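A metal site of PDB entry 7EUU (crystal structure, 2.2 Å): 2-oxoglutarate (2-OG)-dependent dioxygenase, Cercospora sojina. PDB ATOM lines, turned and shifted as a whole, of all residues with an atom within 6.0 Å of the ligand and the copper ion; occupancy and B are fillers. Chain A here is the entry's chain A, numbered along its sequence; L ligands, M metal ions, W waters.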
ATOM      1  N   ARG A 140       4.240 -30.134 -18.165  1.00  0.00           N
ATOM      2  CA  ARG A 140       5.574 -30.389 -18.779  1.00  0.00           C
ATOM      3  C   ARG A 140       6.295 -31.443 -17.931  1.00  0.00           C
ATOM      4  O   ARG A 140       6.352 -31.266 -16.695  1.00  0.00           O
ATOM      5  CB  ARG A 140       6.378 -29.094 -18.863  1.00  0.00           C
ATOM      6  CG  ARG A 140       5.532 -27.847 -19.070  1.00  0.00           C
ATOM      7  CD  ARG A 140       6.362 -26.643 -19.475  1.00  0.00           C
ATOM      8  NE  ARG A 140       6.699 -26.645 -20.889  1.00  0.00           N
ATOM      9  CZ  ARG A 140       6.569 -25.590 -21.690  1.00  0.00           C
ATOM     10  NH1 ARG A 140       6.125 -24.451 -21.216  1.00  0.00           N
ATOM     11  NH2 ARG A 140       6.903 -25.698 -22.974  1.00  0.00           N
ATOM     12  N   THR A 164       8.187 -30.899 -23.486  1.00  0.00           N
ATOM     13  CA  THR A 164       9.544 -30.564 -23.101  1.00  0.00           C
ATOM     14  C   THR A 164       9.535 -29.182 -22.441  1.00  0.00           C
ATOM     15  O   THR A 164       8.542 -28.458 -22.509  1.00  0.00           O
ATOM     16  CB  THR A 164      10.432 -30.602 -24.339  1.00  0.00           C
ATOM     17  OG1 THR A 164      11.788 -30.890 -23.975  1.00  0.00           O
ATOM     18  CG2 THR A 164      10.373 -29.292 -25.087  1.00  0.00           C
ATOM     19  N   PRO A 165      10.612 -28.793 -21.749  1.00  0.00           N
ATOM     20  CA  PRO A 165      10.658 -27.439 -21.181  1.00  0.00           C
ATOM     21  C   PRO A 165      10.655 -26.375 -22.270  1.00  0.00           C
ATOM     22  O   PRO A 165      10.989 -26.620 -23.428  1.00  0.00           O
ATOM     23  CB  PRO A 165      11.964 -27.419 -20.388  1.00  0.00           C
ATOM     24  CG  PRO A 165      12.269 -28.848 -20.124  1.00  0.00           C
ATOM     25  CD  PRO A 165      11.749 -29.609 -21.297  1.00  0.00           C
ATOM     26  N   GLY A 166      10.254 -25.171 -21.876  1.00  0.00           N
ATOM     27  CA  GLY A 166      10.180 -24.062 -22.808  1.00  0.00           C
ATOM     28  C   GLY A 166      11.486 -23.297 -22.925  1.00  0.00           C
ATOM     29  O   GLY A 166      11.668 -22.271 -22.272  1.00  0.00           O
ATOM     30  N   ARG A 167      12.403 -23.800 -23.752  1.00  0.00           N
ATOM     31  CA  ARG A 167      13.752 -23.265 -23.820  1.00  0.00           C
ATOM     32  C   ARG A 167      13.863 -22.250 -24.962  1.00  0.00           C
ATOM     33  O   ARG A 167      14.544 -22.476 -25.977  1.00  0.00           O
ATOM     34  CB  ARG A 167      14.762 -24.399 -23.964  1.00  0.00           C
ATOM     35  CG  ARG A 167      16.095 -24.109 -23.304  1.00  0.00           C
ATOM     36  CD  ARG A 167      17.108 -25.197 -23.589  1.00  0.00           C
ATOM     37  NE  ARG A 167      17.074 -26.262 -22.591  1.00  0.00           N
ATOM     38  CZ  ARG A 167      17.863 -27.330 -22.598  1.00  0.00           C
ATOM     39  NH1 ARG A 167      18.756 -27.478 -23.572  1.00  0.00           N
ATOM     40  NH2 ARG A 167      17.755 -28.243 -21.652  1.00  0.00           N
ATOM     41  N   HIS A 170      10.371 -15.800 -24.428  1.00  0.00           N
ATOM     42  CA  HIS A 170       9.080 -15.481 -24.999  1.00  0.00           C
ATOM     43  C   HIS A 170       8.191 -14.865 -23.934  1.00  0.00           C
ATOM     44  O   HIS A 170       8.456 -14.968 -22.728  1.00  0.00           O
ATOM     45  CB  HIS A 170       8.405 -16.724 -25.574  1.00  0.00           C
ATOM     46  CG  HIS A 170       7.937 -17.703 -24.536  1.00  0.00           C
ATOM     47  ND1 HIS A 170       8.770 -18.666 -23.997  1.00  0.00           N
ATOM     48  CD2 HIS A 170       6.749 -17.851 -23.922  1.00  0.00           C
ATOM     49  CE1 HIS A 170       8.096 -19.363 -23.102  1.00  0.00           C
ATOM     50  NE2 HIS A 170       6.875 -18.895 -23.034  1.00  0.00           N
ATOM     51  N   VAL A 171       7.135 -14.207 -24.397  1.00  0.00           N
ATOM     52  CA  VAL A 171       5.968 -13.888 -23.578  1.00  0.00           C
ATOM     53  C   VAL A 171       4.789 -14.632 -24.202  1.00  0.00           C
ATOM     54  O   VAL A 171       4.635 -14.627 -25.429  1.00  0.00           O
ATOM     55  CB  VAL A 171       5.701 -12.370 -23.519  1.00  0.00           C
ATOM     56  CG1 VAL A 171       4.665 -12.064 -22.448  1.00  0.00           C
ATOM     57  CG2 VAL A 171       6.994 -11.619 -23.241  1.00  0.00           C
ATOM     58  N   ASP A 172       3.986 -15.271 -23.365  1.00  0.00           N
ATOM     59  CA  ASP A 172       2.936 -16.162 -23.871  1.00  0.00           C
ATOM     60  C   ASP A 172       1.906 -15.430 -24.722  1.00  0.00           C
ATOM     61  O   ASP A 172       1.253 -16.067 -25.552  1.00  0.00           O
ATOM     62  CB  ASP A 172       2.249 -16.872 -22.712  1.00  0.00           C
ATOM     63  CG  ASP A 172       3.063 -18.023 -22.162  1.00  0.00           C
ATOM     64  OD1 ASP A 172       4.300 -17.869 -22.052  1.00  0.00           O
ATOM     65  OD2 ASP A 172       2.474 -19.069 -21.843  1.00  0.00           O
ATOM     66  N   ASN A 203       0.377 -16.254 -15.693  1.00  0.00           N
ATOM     67  CA  ASN A 203       0.621 -17.689 -15.648  1.00  0.00           C
ATOM     68  C   ASN A 203       1.086 -18.076 -14.248  1.00  0.00           C
ATOM     69  O   ASN A 203       1.914 -17.380 -13.645  1.00  0.00           O
ATOM     70  CB  ASN A 203       1.666 -18.112 -16.673  1.00  0.00           C
ATOM     71  CG  ASN A 203       1.057 -18.469 -18.019  1.00  0.00           C
ATOM     72  OD1 ASN A 203      -0.054 -18.049 -18.331  1.00  0.00           O
ATOM     73  ND2 ASN A 203       1.792 -19.229 -18.822  1.00  0.00           N
ATOM     74  N   TRP A 205       2.969 -20.885 -12.402  1.00  0.00           N
ATOM     75  CA  TRP A 205       3.877 -21.989 -12.675  1.00  0.00           C
ATOM     76  C   TRP A 205       4.224 -22.690 -11.357  1.00  0.00           C
ATOM     77  O   TRP A 205       4.701 -22.050 -10.418  1.00  0.00           O
ATOM     78  CB  TRP A 205       5.142 -21.452 -13.348  1.00  0.00           C
ATOM     79  CG  TRP A 205       6.086 -22.502 -13.858  1.00  0.00           C
ATOM     80  CD1 TRP A 205       6.114 -23.045 -15.111  1.00  0.00           C
ATOM     81  CD2 TRP A 205       7.164 -23.117 -13.129  1.00  0.00           C
ATOM     82  NE1 TRP A 205       7.133 -23.962 -15.210  1.00  0.00           N
ATOM     83  CE2 TRP A 205       7.786 -24.028 -14.003  1.00  0.00           C
ATOM     84  CE3 TRP A 205       7.644 -22.987 -11.832  1.00  0.00           C
ATOM     85  CZ2 TRP A 205       8.877 -24.809 -13.616  1.00  0.00           C
ATOM     86  CZ3 TRP A 205       8.726 -23.766 -11.447  1.00  0.00           C
ATOM     87  CH2 TRP A 205       9.334 -24.662 -12.334  1.00  0.00           C
ATOM     88  N   GLU A 214      16.553 -27.933 -14.909  1.00  0.00           N
ATOM     89  CA  GLU A 214      15.829 -27.078 -15.839  1.00  0.00           C
ATOM     90  C   GLU A 214      14.811 -26.166 -15.145  1.00  0.00           C
ATOM     91  O   GLU A 214      13.599 -26.300 -15.351  1.00  0.00           O
ATOM     92  CB  GLU A 214      15.148 -27.904 -16.933  1.00  0.00           C
ATOM     93  CG  GLU A 214      14.723 -27.090 -18.150  1.00  0.00           C
ATOM     94  CD  GLU A 214      15.641 -27.291 -19.342  1.00  0.00           C
ATOM     95  OE1 GLU A 214      16.296 -28.347 -19.429  1.00  0.00           O
ATOM     96  OE2 GLU A 214      15.686 -26.388 -20.205  1.00  0.00           O
ATOM     97  N   PRO A 215      15.269 -25.225 -14.308  1.00  0.00           N
ATOM     98  CA  PRO A 215      14.343 -24.284 -13.671  1.00  0.00           C
ATOM     99  C   PRO A 215      13.802 -23.256 -14.663  1.00  0.00           C
ATOM    100  O   PRO A 215      14.178 -23.273 -15.838  1.00  0.00           O
ATOM    101  CB  PRO A 215      15.186 -23.631 -12.583  1.00  0.00           C
ATOM    102  CG  PRO A 215      16.572 -23.681 -13.128  1.00  0.00           C
ATOM    103  CD  PRO A 215      16.665 -24.965 -13.901  1.00  0.00           C
ATOM    104  N   LEU A 216      12.939 -22.366 -14.197  1.00  0.00           N
ATOM    105  CA  LEU A 216      12.311 -21.353 -15.029  1.00  0.00           C
ATOM    106  C   LEU A 216      12.834 -19.972 -14.648  1.00  0.00           C
ATOM    107  O   LEU A 216      12.791 -19.593 -13.475  1.00  0.00           O
ATOM    108  CB  LEU A 216      10.787 -21.392 -14.899  1.00  0.00           C
ATOM    109  CG  LEU A 216       9.995 -20.524 -15.874  1.00  0.00           C
ATOM    110  CD1 LEU A 216      10.302 -20.923 -17.310  1.00  0.00           C
ATOM    111  CD2 LEU A 216       8.518 -20.652 -15.592  1.00  0.00           C
ATOM    112  N   MET A 250       2.321 -14.647 -29.632  1.00  0.00           N
ATOM    113  CA  MET A 250       3.310 -14.448 -28.587  1.00  0.00           C
ATOM    114  C   MET A 250       4.173 -13.226 -28.878  1.00  0.00           C
ATOM    115  O   MET A 250       4.145 -12.649 -29.971  1.00  0.00           O
ATOM    116  CB  MET A 250       4.218 -15.685 -28.462  1.00  0.00           C
ATOM    117  CG  MET A 250       3.585 -16.914 -27.848  1.00  0.00           C
ATOM    118  SD  MET A 250       4.844 -18.170 -27.521  1.00  0.00           S
ATOM    119  CE  MET A 250       4.077 -19.107 -26.196  1.00  0.00           C
ATOM    120  N   ILE A 278       3.707 -15.238 -13.339  1.00  0.00           N
ATOM    121  CA  ILE A 278       4.367 -14.576 -14.453  1.00  0.00           C
ATOM    122  C   ILE A 278       3.328 -13.771 -15.217  1.00  0.00           C
ATOM    123  O   ILE A 278       2.356 -14.337 -15.741  1.00  0.00           O
ATOM    124  CB  ILE A 278       5.068 -15.582 -15.380  1.00  0.00           C
ATOM    125  CG1 ILE A 278       5.963 -16.519 -14.576  1.00  0.00           C
ATOM    126  CG2 ILE A 278       5.872 -14.853 -16.449  1.00  0.00           C
ATOM    127  CD1 ILE A 278       6.533 -17.661 -15.372  1.00  0.00           C
ATOM    128  N   MET A 280       1.956 -12.033 -18.259  1.00  0.00           N
ATOM    129  CA  MET A 280       2.081 -11.978 -19.708  1.00  0.00           C
ATOM    130  C   MET A 280       1.516 -10.687 -20.280  1.00  0.00           C
ATOM    131  O   MET A 280       2.066 -10.147 -21.251  1.00  0.00           O
ATOM    132  CB  MET A 280       1.367 -13.165 -20.351  1.00  0.00           C
ATOM    133  CG  MET A 280       1.762 -14.513 -19.767  1.00  0.00           C
ATOM    134  SD  MET A 280       3.542 -14.760 -19.813  1.00  0.00           S
ATOM    135  CE  MET A 280       3.664 -16.328 -18.960  1.00  0.00           C
ATOM    136  N   HIS A 294      10.384 -14.799 -20.526  1.00  0.00           N
ATOM    137  CA  HIS A 294      10.748 -15.893 -19.644  1.00  0.00           C
ATOM    138  C   HIS A 294      11.196 -17.074 -20.494  1.00  0.00           C
ATOM    139  O   HIS A 294      10.913 -17.149 -21.686  1.00  0.00           O
ATOM    140  CB  HIS A 294       9.590 -16.293 -18.721  1.00  0.00           C
ATOM    141  CG  HIS A 294       8.366 -16.727 -19.465  1.00  0.00           C
ATOM    142  ND1 HIS A 294       7.504 -15.836 -20.071  1.00  0.00           N
ATOM    143  CD2 HIS A 294       7.857 -17.959 -19.705  1.00  0.00           C
ATOM    144  CE1 HIS A 294       6.524 -16.501 -20.649  1.00  0.00           C
ATOM    145  NE2 HIS A 294       6.712 -17.790 -20.445  1.00  0.00           N
ATOM    146  N   SER A 295      11.919 -17.993 -19.847  1.00  0.00           N
ATOM    147  CA  SER A 295      12.468 -19.151 -20.524  1.00  0.00           C
ATOM    148  C   SER A 295      13.022 -20.100 -19.480  1.00  0.00           C
ATOM    149  O   SER A 295      13.565 -19.658 -18.467  1.00  0.00           O
ATOM    150  CB  SER A 295      13.581 -18.749 -21.507  1.00  0.00           C
ATOM    151  OG  SER A 295      14.208 -19.886 -22.075  1.00  0.00           O
ATOM    152  N   SER A 296      12.853 -21.401 -19.725  1.00  0.00           N
ATOM    153  CA  SER A 296      13.593 -22.361 -18.928  1.00  0.00           C
ATOM    154  C   SER A 296      15.051 -22.369 -19.362  1.00  0.00           C
ATOM    155  O   SER A 296      15.421 -21.830 -20.412  1.00  0.00           O
ATOM    156  CB  SER A 296      12.976 -23.757 -19.065  1.00  0.00           C
ATOM    157  OG  SER A 296      13.274 -24.313 -20.329  1.00  0.00           O
ATOM    158  N   ARG A 307      12.567 -32.492 -14.539  1.00  0.00           N
ATOM    159  CA  ARG A 307      11.663 -31.529 -13.923  1.00  0.00           C
ATOM    160  C   ARG A 307      10.272 -31.660 -14.509  1.00  0.00           C
ATOM    161  O   ARG A 307      10.110 -31.836 -15.719  1.00  0.00           O
ATOM    162  CB  ARG A 307      12.199 -30.108 -14.114  1.00  0.00           C
ATOM    163  CG  ARG A 307      11.332 -29.004 -13.501  1.00  0.00           C
ATOM    164  CD  ARG A 307      10.435 -28.348 -14.555  1.00  0.00           C
ATOM    165  NE  ARG A 307      11.176 -27.396 -15.388  1.00  0.00           N
ATOM    166  CZ  ARG A 307      10.625 -26.693 -16.370  1.00  0.00           C
ATOM    167  NH1 ARG A 307       9.331 -26.833 -16.661  1.00  0.00           N
ATOM    168  NH2 ARG A 307      11.363 -25.855 -17.084  1.00  0.00           N
ATOM    169  N   SER A 309       6.199 -29.908 -14.239  1.00  0.00           N
ATOM    170  CA  SER A 309       5.522 -28.700 -13.795  1.00  0.00           C
ATOM    171  C   SER A 309       4.204 -28.565 -14.531  1.00  0.00           C
ATOM    172  O   SER A 309       3.968 -29.215 -15.555  1.00  0.00           O
ATOM    173  CB  SER A 309       6.382 -27.461 -14.030  1.00  0.00           C
ATOM    174  OG  SER A 309       6.710 -27.333 -15.412  1.00  0.00           O
ATOM    175  N   GLU A 311       1.801 -25.096 -15.816  1.00  0.00           N
ATOM    176  CA  GLU A 311       1.607 -23.664 -15.920  1.00  0.00           C
ATOM    177  C   GLU A 311       0.133 -23.415 -16.215  1.00  0.00           C
ATOM    178  O   GLU A 311      -0.384 -23.907 -17.216  1.00  0.00           O
ATOM    179  CB  GLU A 311       2.502 -23.053 -16.998  1.00  0.00           C
ATOM    180  CG  GLU A 311       2.398 -23.702 -18.364  1.00  0.00           C
ATOM    181  CD  GLU A 311       3.719 -23.711 -19.109  1.00  0.00           C
ATOM    182  OE1 GLU A 311       4.720 -24.189 -18.535  1.00  0.00           O
ATOM    183  OE2 GLU A 311       3.748 -23.242 -20.267  1.00  0.00           O
ATOM    184  N   ARG A 313      -2.713 -20.895 -17.087  1.00  0.00           N
ATOM    185  CA  ARG A 313      -3.037 -19.597 -17.730  1.00  0.00           C
ATOM    186  C   ARG A 313      -4.269 -19.014 -17.037  1.00  0.00           C
ATOM    187  O   ARG A 313      -5.273 -19.746 -16.889  1.00  0.00           O
ATOM    188  CB  ARG A 313      -3.287 -19.799 -19.227  1.00  0.00           C
ATOM    189  CG  ARG A 313      -2.395 -20.847 -19.875  1.00  0.00           C
ATOM    190  CD  ARG A 313      -1.848 -20.402 -21.213  1.00  0.00           C
ATOM    191  NE  ARG A 313      -0.389 -20.407 -21.245  1.00  0.00           N
ATOM    192  CZ  ARG A 313       0.356 -21.473 -21.518  1.00  0.00           C
ATOM    193  NH1 ARG A 313      -0.225 -22.633 -21.781  1.00  0.00           N
ATOM    194  NH2 ARG A 313       1.669 -21.377 -21.520  1.00  0.00           N
HETATM  195  C1  LIG L   1       5.268 -20.761 -19.012  1.00  0.00           C
HETATM  196  C2  LIG L   1       6.591 -21.288 -19.574  1.00  0.00           C
HETATM  197  C3  LIG L   1       8.336 -23.092 -19.647  1.00  0.00           C
HETATM  198  C4  LIG L   1       8.773 -24.284 -18.801  1.00  0.00           C
HETATM  199  O1  LIG L   1       4.858 -21.163 -17.897  1.00  0.00           O
HETATM  200  O2  LIG L   1       4.596 -19.919 -19.677  1.00  0.00           O
HETATM  201  O3  LIG L   1       7.184 -20.655 -20.370  1.00  0.00           O
HETATM  202  O4  LIG L   1       9.749 -24.989 -19.168  1.00  0.00           O
HETATM  203  N1  LIG L   1       7.088 -22.578 -19.125  1.00  0.00           N
HETATM  204  O5  LIG L   1       8.144 -24.560 -17.743  1.00  0.00           O
HETATM  205 CU    CU M   1       5.739 -19.270 -21.360  1.00  0.00          CU
HETATM  206  O   HOH W   1       4.553 -20.886 -22.423  1.00  0.00           O
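The guanidinium group (NE) of Arg 140 is in salt-bridge range of an oxygen (O4) of the ligand, at 3.9 Å. N of Gly 166 sits at hydrogen-bond distance from O4 of the ligand, at 2.8 Å. An oxygen (O4) of the ligand is in salt-bridge range of the guanidinium group (NH2) of Arg 307 (2.8 Å). An oxygen (O5) of the ligand lies within hydrogen-bond range of the indole nitrogen of Trp 205, 2.8 Å away. O2 of the ligand lies close to NH2 of Arg 313 (3.8 Å). An oxygen (O2) of the ligand sits close to the side-chain amide nitrogen (ND2) of Asn 203. OE1 of Glu 311 is in hydrogen-bond range of N1 of the ligand.
The backbone NH (N) of Asp 172 is in hydrogen-bond range of the side-chain sulfur (SD) of Met 280, at 3.6 Å. OE2 of Glu 311 lies within salt-bridge range of NH1 of Arg 140 (2.8 Å). The side-chain hydroxyl of Ser 296 sits at hydrogen-bond distance from the side-chain carboxylate of Glu 214 (3.2 Å). The backbone NH of Arg 140 lies within hydrogen-bond range of the backbone carbonyl oxygen of Ser 309 (2.8 Å). OG of Ser 309 lies within hydrogen-bond range of NH1 of Arg 307, at 2.9 Å. The guanidinium group (NE) of Arg 140 lies within hydrogen-bond range of the backbone carbonyl oxygen (O) of Thr 164 (3.1 Å). NE of Arg 307 is in hydrogen-bond range of O of Glu 214, 2.7 Å away. The backbone carbonyl oxygen (O) of Gly 166 is in hydrogen-bond range of the backbone NH (N) of Ser 296 (2.9 Å).
Pro 165 touches the ligand (CA to O4, 3.3 Å). Leu 216 touches the ligand. CE of Met 280 touches O2 of the ligand, at 3.8 Å. CB of Ser 296 touches O4 of the ligand, at 3.5 Å. OG of Ser 309 touches O5 of the ligand (3.9 Å).
Within 4 Å of the copper ion: His 170, Asp 172 and His 294.
The copper ion is bound by a ring nitrogen (NE2) of His 294, a ring nitrogen (NE2) of His 170, the side-chain carboxylate (OD1) of Asp 172, an oxygen (O2) of the ligand, an oxygen (O3) of the ligand and water W1.
Water W1 lies within hydrogen-bond range of the side-chain carboxylate of Asp 172, the guanidinium group of Arg 313 and the side-chain carboxylate of Glu 311.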
